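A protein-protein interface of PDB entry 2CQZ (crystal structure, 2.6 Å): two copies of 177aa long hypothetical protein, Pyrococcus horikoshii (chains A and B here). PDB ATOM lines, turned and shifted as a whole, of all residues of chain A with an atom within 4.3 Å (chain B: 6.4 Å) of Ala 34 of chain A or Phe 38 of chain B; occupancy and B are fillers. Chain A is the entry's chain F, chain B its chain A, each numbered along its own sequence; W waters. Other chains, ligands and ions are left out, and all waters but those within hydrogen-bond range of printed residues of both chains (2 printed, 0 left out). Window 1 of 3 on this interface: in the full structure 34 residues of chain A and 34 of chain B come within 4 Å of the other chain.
The side-chain hydroxyl (OG) of Ser 32 of chain A is in hydrogen-bond range of the side-chain carboxylate (OD1) of Asp 35 of chain B, at 2.5 Å. The backbone NH of Asp 35 of chain B lies within hydrogen-bond range of the side-chain carboxylate of Asp 35 of chain A. NZ of Lys 15 of chain A lies within salt-bridge range of OD1 of Asp 130 of chain B (2.8 Å).
ND1 of His 36 of chain B sits at hydrogen-bond distance from OD2 of Asp 130 of chain B. OG of Ser 37 of chain A is in hydrogen-bond range of O of Ile 33 of chain A (3.0 Å). The side-chain hydroxyl (OG) of Ser 32 of chain A sits close to the backbone NH (N) of Ala 34 of chain A, 3.3 Å away. The backbone NH of Ile 33 of chain A sits at hydrogen-bond distance from the backbone carbonyl oxygen of Leu 14 of chain A. The side-chain hydroxyl (OG) of Ser 37 of chain B sits at hydrogen-bond distance from the backbone carbonyl oxygen (O) of Ile 33 of chain B. The backbone NH (N) of Ser 32 of chain A lies within hydrogen-bond range of the side-chain carboxylate (OD2) of Asp 35 of chain A (3.0 Å).
CG1 of Val 11 of chain A touches CE1 of Phe 38 of chain B (3.8 Å). Lys 15 of chain A touches Asp 35 of chain B (CA to OD1, 3.6 Å). CB of Ala 34 of chain A touches OD1 of Asp 35 of chain B, 3.2 Å away. Ala 34 of chain A touches Phe 38 of chain B. OD1 of Asp 35 of chain A touches CB of Ala 34 of chain B, at 3.3 Å. Ser 37 of chain A touches Phe 38 of chain B (CB to CE2, 3.5 Å). Ala 34 of chain B touches Phe 38 of chain A (O to CB, 3.6 Å). Phe 38 of chain A touches Ser 37 of chain B. Phe 38 of chain B touches Ile 68 of chain A. Ile 68 of chain A touches Ala 41 of chain B.
Of chain B, only Asp 35 (3.2 Å) and Phe 38 (3.6 Å) come within 4 Å of Ala 34 of chain A. Printed residues of chain A within 4 Å of Asp 35 of chain B: Lys 15, Ser 32, Ala 34 and Asp 35. Of the printed residues of chain A, Ala 41 of chain B touches Ile 68. Val 40 of chain B touches none of the printed residues of chain A. His 36 of chain A touches none of the printed residues of chain B. The nearest printed residue of chain A that does not touch Phe 38 of chain B is Phe 38 of chain A (4.3 Å). The nearest printed residue of chain A that does not touch Ala 34 of chain B is Ala 34 of chain A (4.4 Å).
Of the 12 printed residues of chain B, 7 touch a printed residue of chain A. Hydrophobic or aromatic side chains of chain B that line the printed part of chain A: Ala 34, Phe 38, Ala 41 and Phe 42. Hydrophobic or aromatic side chains of chain A that line the printed part of chain B: Val 11, Leu 14, Ala 34, Phe 38 and Ile 68. Among the printed residues, Asp or Glu carboxylates within 4 Å of a Lys or Arg side-chain nitrogen of the other chain: Lys 15 of chain A with Asp 130 of chain B (2.8 Å).
Ala 34 of chain A touches Asp 35 of chain B, and with the chains exchanged Asp 35 of chain A touches Ala 34 of chain B. Ala 34 of chain A touches Phe 38 of chain B, and with the chains exchanged Phe 38 of chain A touches Ala 34 of chain B. Asp 35 of chain A touches its own counterpart, Asp 35 of chain B. Ser 37 of chain A touches Phe 38 of chain B, and with the chains exchanged Phe 38 of chain A touches Ser 37 of chain B.
Water W1 lies within hydrogen-bond range of the backbone carbonyl oxygen (O) of Lys 15 of chain A (2.5 Å) and the side-chain carboxylate (OD2) of Asp 35 of chain B (3.1 Å). Water W2 lies within hydrogen-bond range of the side-chain carboxylate of Asp 35 of chain A and the side-chain carboxylate of Asp 35 of chain B.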
ATOM      1  N   VAL A  11      16.664 -37.380  32.185  1.00  0.00           N
ATOM      2  CA  VAL A  11      17.587 -36.734  31.253  1.00  0.00           C
ATOM      3  C   VAL A  11      17.882 -35.283  31.651  1.00  0.00           C
ATOM      4  O   VAL A  11      18.898 -34.707  31.287  1.00  0.00           O
ATOM      5  CB  VAL A  11      16.962 -36.775  29.858  1.00  0.00           C
ATOM      6  CG1 VAL A  11      17.778 -35.914  28.897  1.00  0.00           C
ATOM      7  CG2 VAL A  11      16.930 -38.203  29.345  1.00  0.00           C
ATOM      8  N   LEU A  14      21.116 -34.028  33.342  1.00  0.00           N
ATOM      9  CA  LEU A  14      22.218 -33.546  32.512  1.00  0.00           C
ATOM     10  C   LEU A  14      22.505 -32.058  32.701  1.00  0.00           C
ATOM     11  O   LEU A  14      23.652 -31.625  32.565  1.00  0.00           O
ATOM     12  CB  LEU A  14      21.921 -33.831  31.039  1.00  0.00           C
ATOM     13  CG  LEU A  14      21.985 -35.307  30.653  1.00  0.00           C
ATOM     14  CD1 LEU A  14      21.714 -35.469  29.169  1.00  0.00           C
ATOM     15  CD2 LEU A  14      23.360 -35.855  31.011  1.00  0.00           C
ATOM     16  N   LYS A  15      21.464 -31.283  32.999  1.00  0.00           N
ATOM     17  CA  LYS A  15      21.632 -29.849  33.252  1.00  0.00           C
ATOM     18  C   LYS A  15      22.458 -29.612  34.514  1.00  0.00           C
ATOM     19  O   LYS A  15      23.025 -28.550  34.742  1.00  0.00           O
ATOM     20  CB  LYS A  15      20.256 -29.220  33.496  1.00  0.00           C
ATOM     21  CG  LYS A  15      19.266 -29.332  32.335  1.00  0.00           C
ATOM     22  CD  LYS A  15      18.026 -28.474  32.595  1.00  0.00           C
ATOM     23  CE  LYS A  15      16.918 -28.649  31.548  1.00  0.00           C
ATOM     24  NZ  LYS A  15      15.891 -27.624  31.765  1.00  0.00           N
ATOM     25  N   SER A  32      27.619 -27.761  31.733  1.00  0.00           N
ATOM     26  CA  SER A  32      26.947 -28.997  32.089  1.00  0.00           C
ATOM     27  C   SER A  32      26.951 -29.923  30.862  1.00  0.00           C
ATOM     28  O   SER A  32      27.324 -29.511  29.767  1.00  0.00           O
ATOM     29  CB  SER A  32      25.504 -28.693  32.514  1.00  0.00           C
ATOM     30  OG  SER A  32      24.700 -28.314  31.404  1.00  0.00           O
ATOM     31  N   ILE A  33      26.535 -31.171  31.037  1.00  0.00           N
ATOM     32  CA  ILE A  33      26.497 -32.095  29.905  1.00  0.00           C
ATOM     33  C   ILE A  33      25.432 -31.629  28.913  1.00  0.00           C
ATOM     34  O   ILE A  33      25.566 -31.824  27.699  1.00  0.00           O
ATOM     35  CB  ILE A  33      26.181 -33.543  30.373  1.00  0.00           C
ATOM     36  CG1 ILE A  33      27.263 -34.014  31.351  1.00  0.00           C
ATOM     37  CG2 ILE A  33      26.101 -34.481  29.179  1.00  0.00           C
ATOM     38  CD1 ILE A  33      26.912 -35.304  32.088  1.00  0.00           C
ATOM     39  N   ALA A  34      24.377 -31.011  29.448  1.00  0.00           N
ATOM     40  CA  ALA A  34      23.259 -30.495  28.653  1.00  0.00           C
ATOM     41  C   ALA A  34      23.739 -29.345  27.776  1.00  0.00           C
ATOM     42  O   ALA A  34      23.369 -29.263  26.611  1.00  0.00           O
ATOM     43  CB  ALA A  34      22.135 -30.020  29.567  1.00  0.00           C
ATOM     44  N   ASP A  35      24.554 -28.460  28.354  1.00  0.00           N
ATOM     45  CA  ASP A  35      25.130 -27.327  27.632  1.00  0.00           C
ATOM     46  C   ASP A  35      25.904 -27.877  26.454  1.00  0.00           C
ATOM     47  O   ASP A  35      25.742 -27.438  25.311  1.00  0.00           O
ATOM     48  CB  ASP A  35      26.104 -26.548  28.514  1.00  0.00           C
ATOM     49  CG  ASP A  35      25.405 -25.639  29.489  1.00  0.00           C
ATOM     50  OD1 ASP A  35      24.448 -24.947  29.070  1.00  0.00           O
ATOM     51  OD2 ASP A  35      25.818 -25.600  30.668  1.00  0.00           O
ATOM     52  N   HIS A  36      26.763 -28.845  26.746  1.00  0.00           N
ATOM     53  CA  HIS A  36      27.564 -29.467  25.713  1.00  0.00           C
ATOM     54  C   HIS A  36      26.678 -30.102  24.630  1.00  0.00           C
ATOM     55  O   HIS A  36      26.929 -29.913  23.436  1.00  0.00           O
ATOM     56  CB  HIS A  36      28.485 -30.507  26.336  1.00  0.00           C
ATOM     57  CG  HIS A  36      29.104 -31.423  25.339  1.00  0.00           C
ATOM     58  ND1 HIS A  36      29.963 -30.981  24.355  1.00  0.00           N
ATOM     59  CD2 HIS A  36      28.939 -32.750  25.126  1.00  0.00           C
ATOM     60  CE1 HIS A  36      30.298 -31.994  23.577  1.00  0.00           C
ATOM     61  NE2 HIS A  36      29.689 -33.078  24.024  1.00  0.00           N
ATOM     62  N   SER A  37      25.643 -30.839  25.036  1.00  0.00           N
ATOM     63  CA  SER A  37      24.751 -31.477  24.063  1.00  0.00           C
ATOM     64  C   SER A  37      24.051 -30.467  23.159  1.00  0.00           C
ATOM     65  O   SER A  37      23.874 -30.714  21.970  1.00  0.00           O
ATOM     66  CB  SER A  37      23.696 -32.334  24.765  1.00  0.00           C
ATOM     67  OG  SER A  37      24.294 -33.415  25.452  1.00  0.00           O
ATOM     68  N   PHE A  38      23.633 -29.339  23.725  1.00  0.00           N
ATOM     69  CA  PHE A  38      22.982 -28.316  22.921  1.00  0.00           C
ATOM     70  C   PHE A  38      23.948 -27.893  21.825  1.00  0.00           C
ATOM     71  O   PHE A  38      23.592 -27.895  20.649  1.00  0.00           O
ATOM     72  CB  PHE A  38      22.596 -27.078  23.753  1.00  0.00           C
ATOM     73  CG  PHE A  38      22.101 -25.927  22.906  1.00  0.00           C
ATOM     74  CD1 PHE A  38      22.904 -24.808  22.677  1.00  0.00           C
ATOM     75  CD2 PHE A  38      20.868 -26.008  22.250  1.00  0.00           C
ATOM     76  CE1 PHE A  38      22.485 -23.782  21.794  1.00  0.00           C
ATOM     77  CE2 PHE A  38      20.445 -24.998  21.373  1.00  0.00           C
ATOM     78  CZ  PHE A  38      21.257 -23.883  21.142  1.00  0.00           C
ATOM     79  N   ILE A  68      21.319 -35.331  19.885  1.00  0.00           N
ATOM     80  CA  ILE A  68      20.565 -35.082  21.104  1.00  0.00           C
ATOM     81  C   ILE A  68      20.768 -36.162  22.170  1.00  0.00           C
ATOM     82  O   ILE A  68      20.885 -35.872  23.357  1.00  0.00           O
ATOM     83  CB  ILE A  68      19.052 -34.941  20.781  1.00  0.00           C
ATOM     84  CG1 ILE A  68      18.817 -33.612  20.057  1.00  0.00           C
ATOM     85  CG2 ILE A  68      18.219 -35.023  22.045  1.00  0.00           C
ATOM     86  CD1 ILE A  68      17.423 -33.446  19.479  1.00  0.00           C
ATOM     87  N   ILE B  33      20.535 -20.835  29.229  1.00  0.00           N
ATOM     88  CA  ILE B  33      19.579 -20.901  28.141  1.00  0.00           C
ATOM     89  C   ILE B  33      19.847 -22.175  27.340  1.00  0.00           C
ATOM     90  O   ILE B  33      18.908 -22.820  26.875  1.00  0.00           O
ATOM     91  CB  ILE B  33      19.660 -19.654  27.221  1.00  0.00           C
ATOM     92  CG1 ILE B  33      19.414 -18.384  28.037  1.00  0.00           C
ATOM     93  CG2 ILE B  33      18.622 -19.766  26.116  1.00  0.00           C
ATOM     94  CD1 ILE B  33      19.548 -17.111  27.256  1.00  0.00           C
ATOM     95  N   ALA B  34      21.121 -22.545  27.194  1.00  0.00           N
ATOM     96  CA  ALA B  34      21.485 -23.770  26.466  1.00  0.00           C
ATOM     97  C   ALA B  34      20.952 -25.021  27.180  1.00  0.00           C
ATOM     98  O   ALA B  34      20.506 -25.956  26.518  1.00  0.00           O
ATOM     99  CB  ALA B  34      22.989 -23.869  26.299  1.00  0.00           C
ATOM    100  N   ASP B  35      21.003 -25.048  28.519  1.00  0.00           N
ATOM    101  CA  ASP B  35      20.468 -26.189  29.280  1.00  0.00           C
ATOM    102  C   ASP B  35      19.005 -26.352  28.889  1.00  0.00           C
ATOM    103  O   ASP B  35      18.539 -27.441  28.548  1.00  0.00           O
ATOM    104  CB  ASP B  35      20.504 -25.932  30.790  1.00  0.00           C
ATOM    105  CG  ASP B  35      21.862 -26.160  31.398  1.00  0.00           C
ATOM    106  OD1 ASP B  35      22.513 -27.150  31.014  1.00  0.00           O
ATOM    107  OD2 ASP B  35      22.259 -25.360  32.274  1.00  0.00           O
ATOM    108  N   HIS B  36      18.288 -25.237  28.957  1.00  0.00           N
ATOM    109  CA  HIS B  36      16.879 -25.183  28.620  1.00  0.00           C
ATOM    110  C   HIS B  36      16.632 -25.699  27.204  1.00  0.00           C
ATOM    111  O   HIS B  36      15.796 -26.580  26.997  1.00  0.00           O
ATOM    112  CB  HIS B  36      16.385 -23.737  28.763  1.00  0.00           C
ATOM    113  CG  HIS B  36      15.008 -23.511  28.227  1.00  0.00           C
ATOM    114  ND1 HIS B  36      13.922 -24.261  28.624  1.00  0.00           N
ATOM    115  CD2 HIS B  36      14.545 -22.645  27.293  1.00  0.00           C
ATOM    116  CE1 HIS B  36      12.851 -23.871  27.955  1.00  0.00           C
ATOM    117  NE2 HIS B  36      13.203 -22.893  27.142  1.00  0.00           N
ATOM    118  N   SER B  37      17.368 -25.160  26.234  1.00  0.00           N
ATOM    119  CA  SER B  37      17.200 -25.560  24.841  1.00  0.00           C
ATOM    120  C   SER B  37      17.428 -27.045  24.658  1.00  0.00           C
ATOM    121  O   SER B  37      16.737 -27.689  23.866  1.00  0.00           O
ATOM    122  CB  SER B  37      18.143 -24.760  23.925  1.00  0.00           C
ATOM    123  OG  SER B  37      17.796 -23.378  23.906  1.00  0.00           O
ATOM    124  N   PHE B  38      18.396 -27.603  25.379  1.00  0.00           N
ATOM    125  CA  PHE B  38      18.609 -29.024  25.217  1.00  0.00           C
ATOM    126  C   PHE B  38      17.374 -29.784  25.666  1.00  0.00           C
ATOM    127  O   PHE B  38      16.917 -30.715  25.018  1.00  0.00           O
ATOM    128  CB  PHE B  38      19.809 -29.430  26.073  1.00  0.00           C
ATOM    129  CG  PHE B  38      19.907 -30.927  26.120  1.00  0.00           C
ATOM    130  CD1 PHE B  38      19.574 -31.601  27.288  1.00  0.00           C
ATOM    131  CD2 PHE B  38      20.272 -31.631  24.985  1.00  0.00           C
ATOM    132  CE1 PHE B  38      19.596 -32.988  27.313  1.00  0.00           C
ATOM    133  CE2 PHE B  38      20.293 -33.022  25.017  1.00  0.00           C
ATOM    134  CZ  PHE B  38      19.952 -33.706  26.178  1.00  0.00           C
ATOM    135  N   GLY B  39      16.796 -29.377  26.793  1.00  0.00           N
ATOM    136  CA  GLY B  39      15.588 -30.011  27.277  1.00  0.00           C
ATOM    137  C   GLY B  39      14.461 -29.912  26.264  1.00  0.00           C
ATOM    138  O   GLY B  39      13.808 -30.914  25.944  1.00  0.00           O
ATOM    139  N   VAL B  40      14.223 -28.705  25.754  1.00  0.00           N
ATOM    140  CA  VAL B  40      13.171 -28.515  24.766  1.00  0.00           C
ATOM    141  C   VAL B  40      13.422 -29.486  23.605  1.00  0.00           C
ATOM    142  O   VAL B  40      12.501 -30.178  23.154  1.00  0.00           O
ATOM    143  CB  VAL B  40      13.127 -27.046  24.279  1.00  0.00           C
ATOM    144  CG1 VAL B  40      12.121 -26.890  23.172  1.00  0.00           C
ATOM    145  CG2 VAL B  40      12.744 -26.132  25.435  1.00  0.00           C
ATOM    146  N   ALA B  41      14.671 -29.575  23.153  1.00  0.00           N
ATOM    147  CA  ALA B  41      15.011 -30.495  22.067  1.00  0.00           C
ATOM    148  C   ALA B  41      14.714 -31.946  22.425  1.00  0.00           C
ATOM    149  O   ALA B  41      14.200 -32.700  21.599  1.00  0.00           O
ATOM    150  CB  ALA B  41      16.482 -30.356  21.692  1.00  0.00           C
ATOM    151  N   PHE B  42      15.038 -32.349  23.647  1.00  0.00           N
ATOM    152  CA  PHE B  42      14.796 -33.726  24.051  1.00  0.00           C
ATOM    153  C   PHE B  42      13.318 -34.055  24.212  1.00  0.00           C
ATOM    154  O   PHE B  42      12.862 -35.127  23.814  1.00  0.00           O
ATOM    155  CB  PHE B  42      15.518 -34.055  25.355  1.00  0.00           C
ATOM    156  CG  PHE B  42      15.356 -35.485  25.765  1.00  0.00           C
ATOM    157  CD1 PHE B  42      15.932 -36.503  25.010  1.00  0.00           C
ATOM    158  CD2 PHE B  42      14.542 -35.822  26.838  1.00  0.00           C
ATOM    159  CE1 PHE B  42      15.700 -37.824  25.319  1.00  0.00           C
ATOM    160  CE2 PHE B  42      14.307 -37.133  27.151  1.00  0.00           C
ATOM    161  CZ  PHE B  42      14.882 -38.141  26.387  1.00  0.00           C
ATOM    162  N   ILE B  43      12.574 -33.139  24.819  1.00  0.00           N
ATOM    163  CA  ILE B  43      11.148 -33.339  25.006  1.00  0.00           C
ATOM    164  C   ILE B  43      10.477 -33.382  23.629  1.00  0.00           C
ATOM    165  O   ILE B  43       9.605 -34.219  23.371  1.00  0.00           O
ATOM    166  CB  ILE B  43      10.543 -32.214  25.873  1.00  0.00           C
ATOM    167  CG1 ILE B  43      11.128 -32.285  27.293  1.00  0.00           C
ATOM    168  CG2 ILE B  43       9.027 -32.338  25.896  1.00  0.00           C
ATOM    169  CD1 ILE B  43      10.690 -31.174  28.220  1.00  0.00           C
ATOM    170  N   ASP B 130       9.525 -28.323  29.720  1.00  0.00           N
ATOM    171  CA  ASP B 130      10.850 -28.231  30.310  1.00  0.00           C
ATOM    172  C   ASP B 130      10.757 -27.234  31.453  1.00  0.00           C
ATOM    173  O   ASP B 130      11.248 -27.484  32.557  1.00  0.00           O
ATOM    174  CB  ASP B 130      11.861 -27.721  29.277  1.00  0.00           C
ATOM    175  CG  ASP B 130      13.256 -27.548  29.852  1.00  0.00           C
ATOM    176  OD1 ASP B 130      13.983 -28.558  29.965  1.00  0.00           O
ATOM    177  OD2 ASP B 130      13.622 -26.402  30.193  1.00  0.00           O
HETATM  178  O   HOH W   1      21.844 -26.377  35.176  1.00  0.00           O
HETATM  179  O   HOH W   2      24.796 -24.697  32.878  1.00  0.00           O
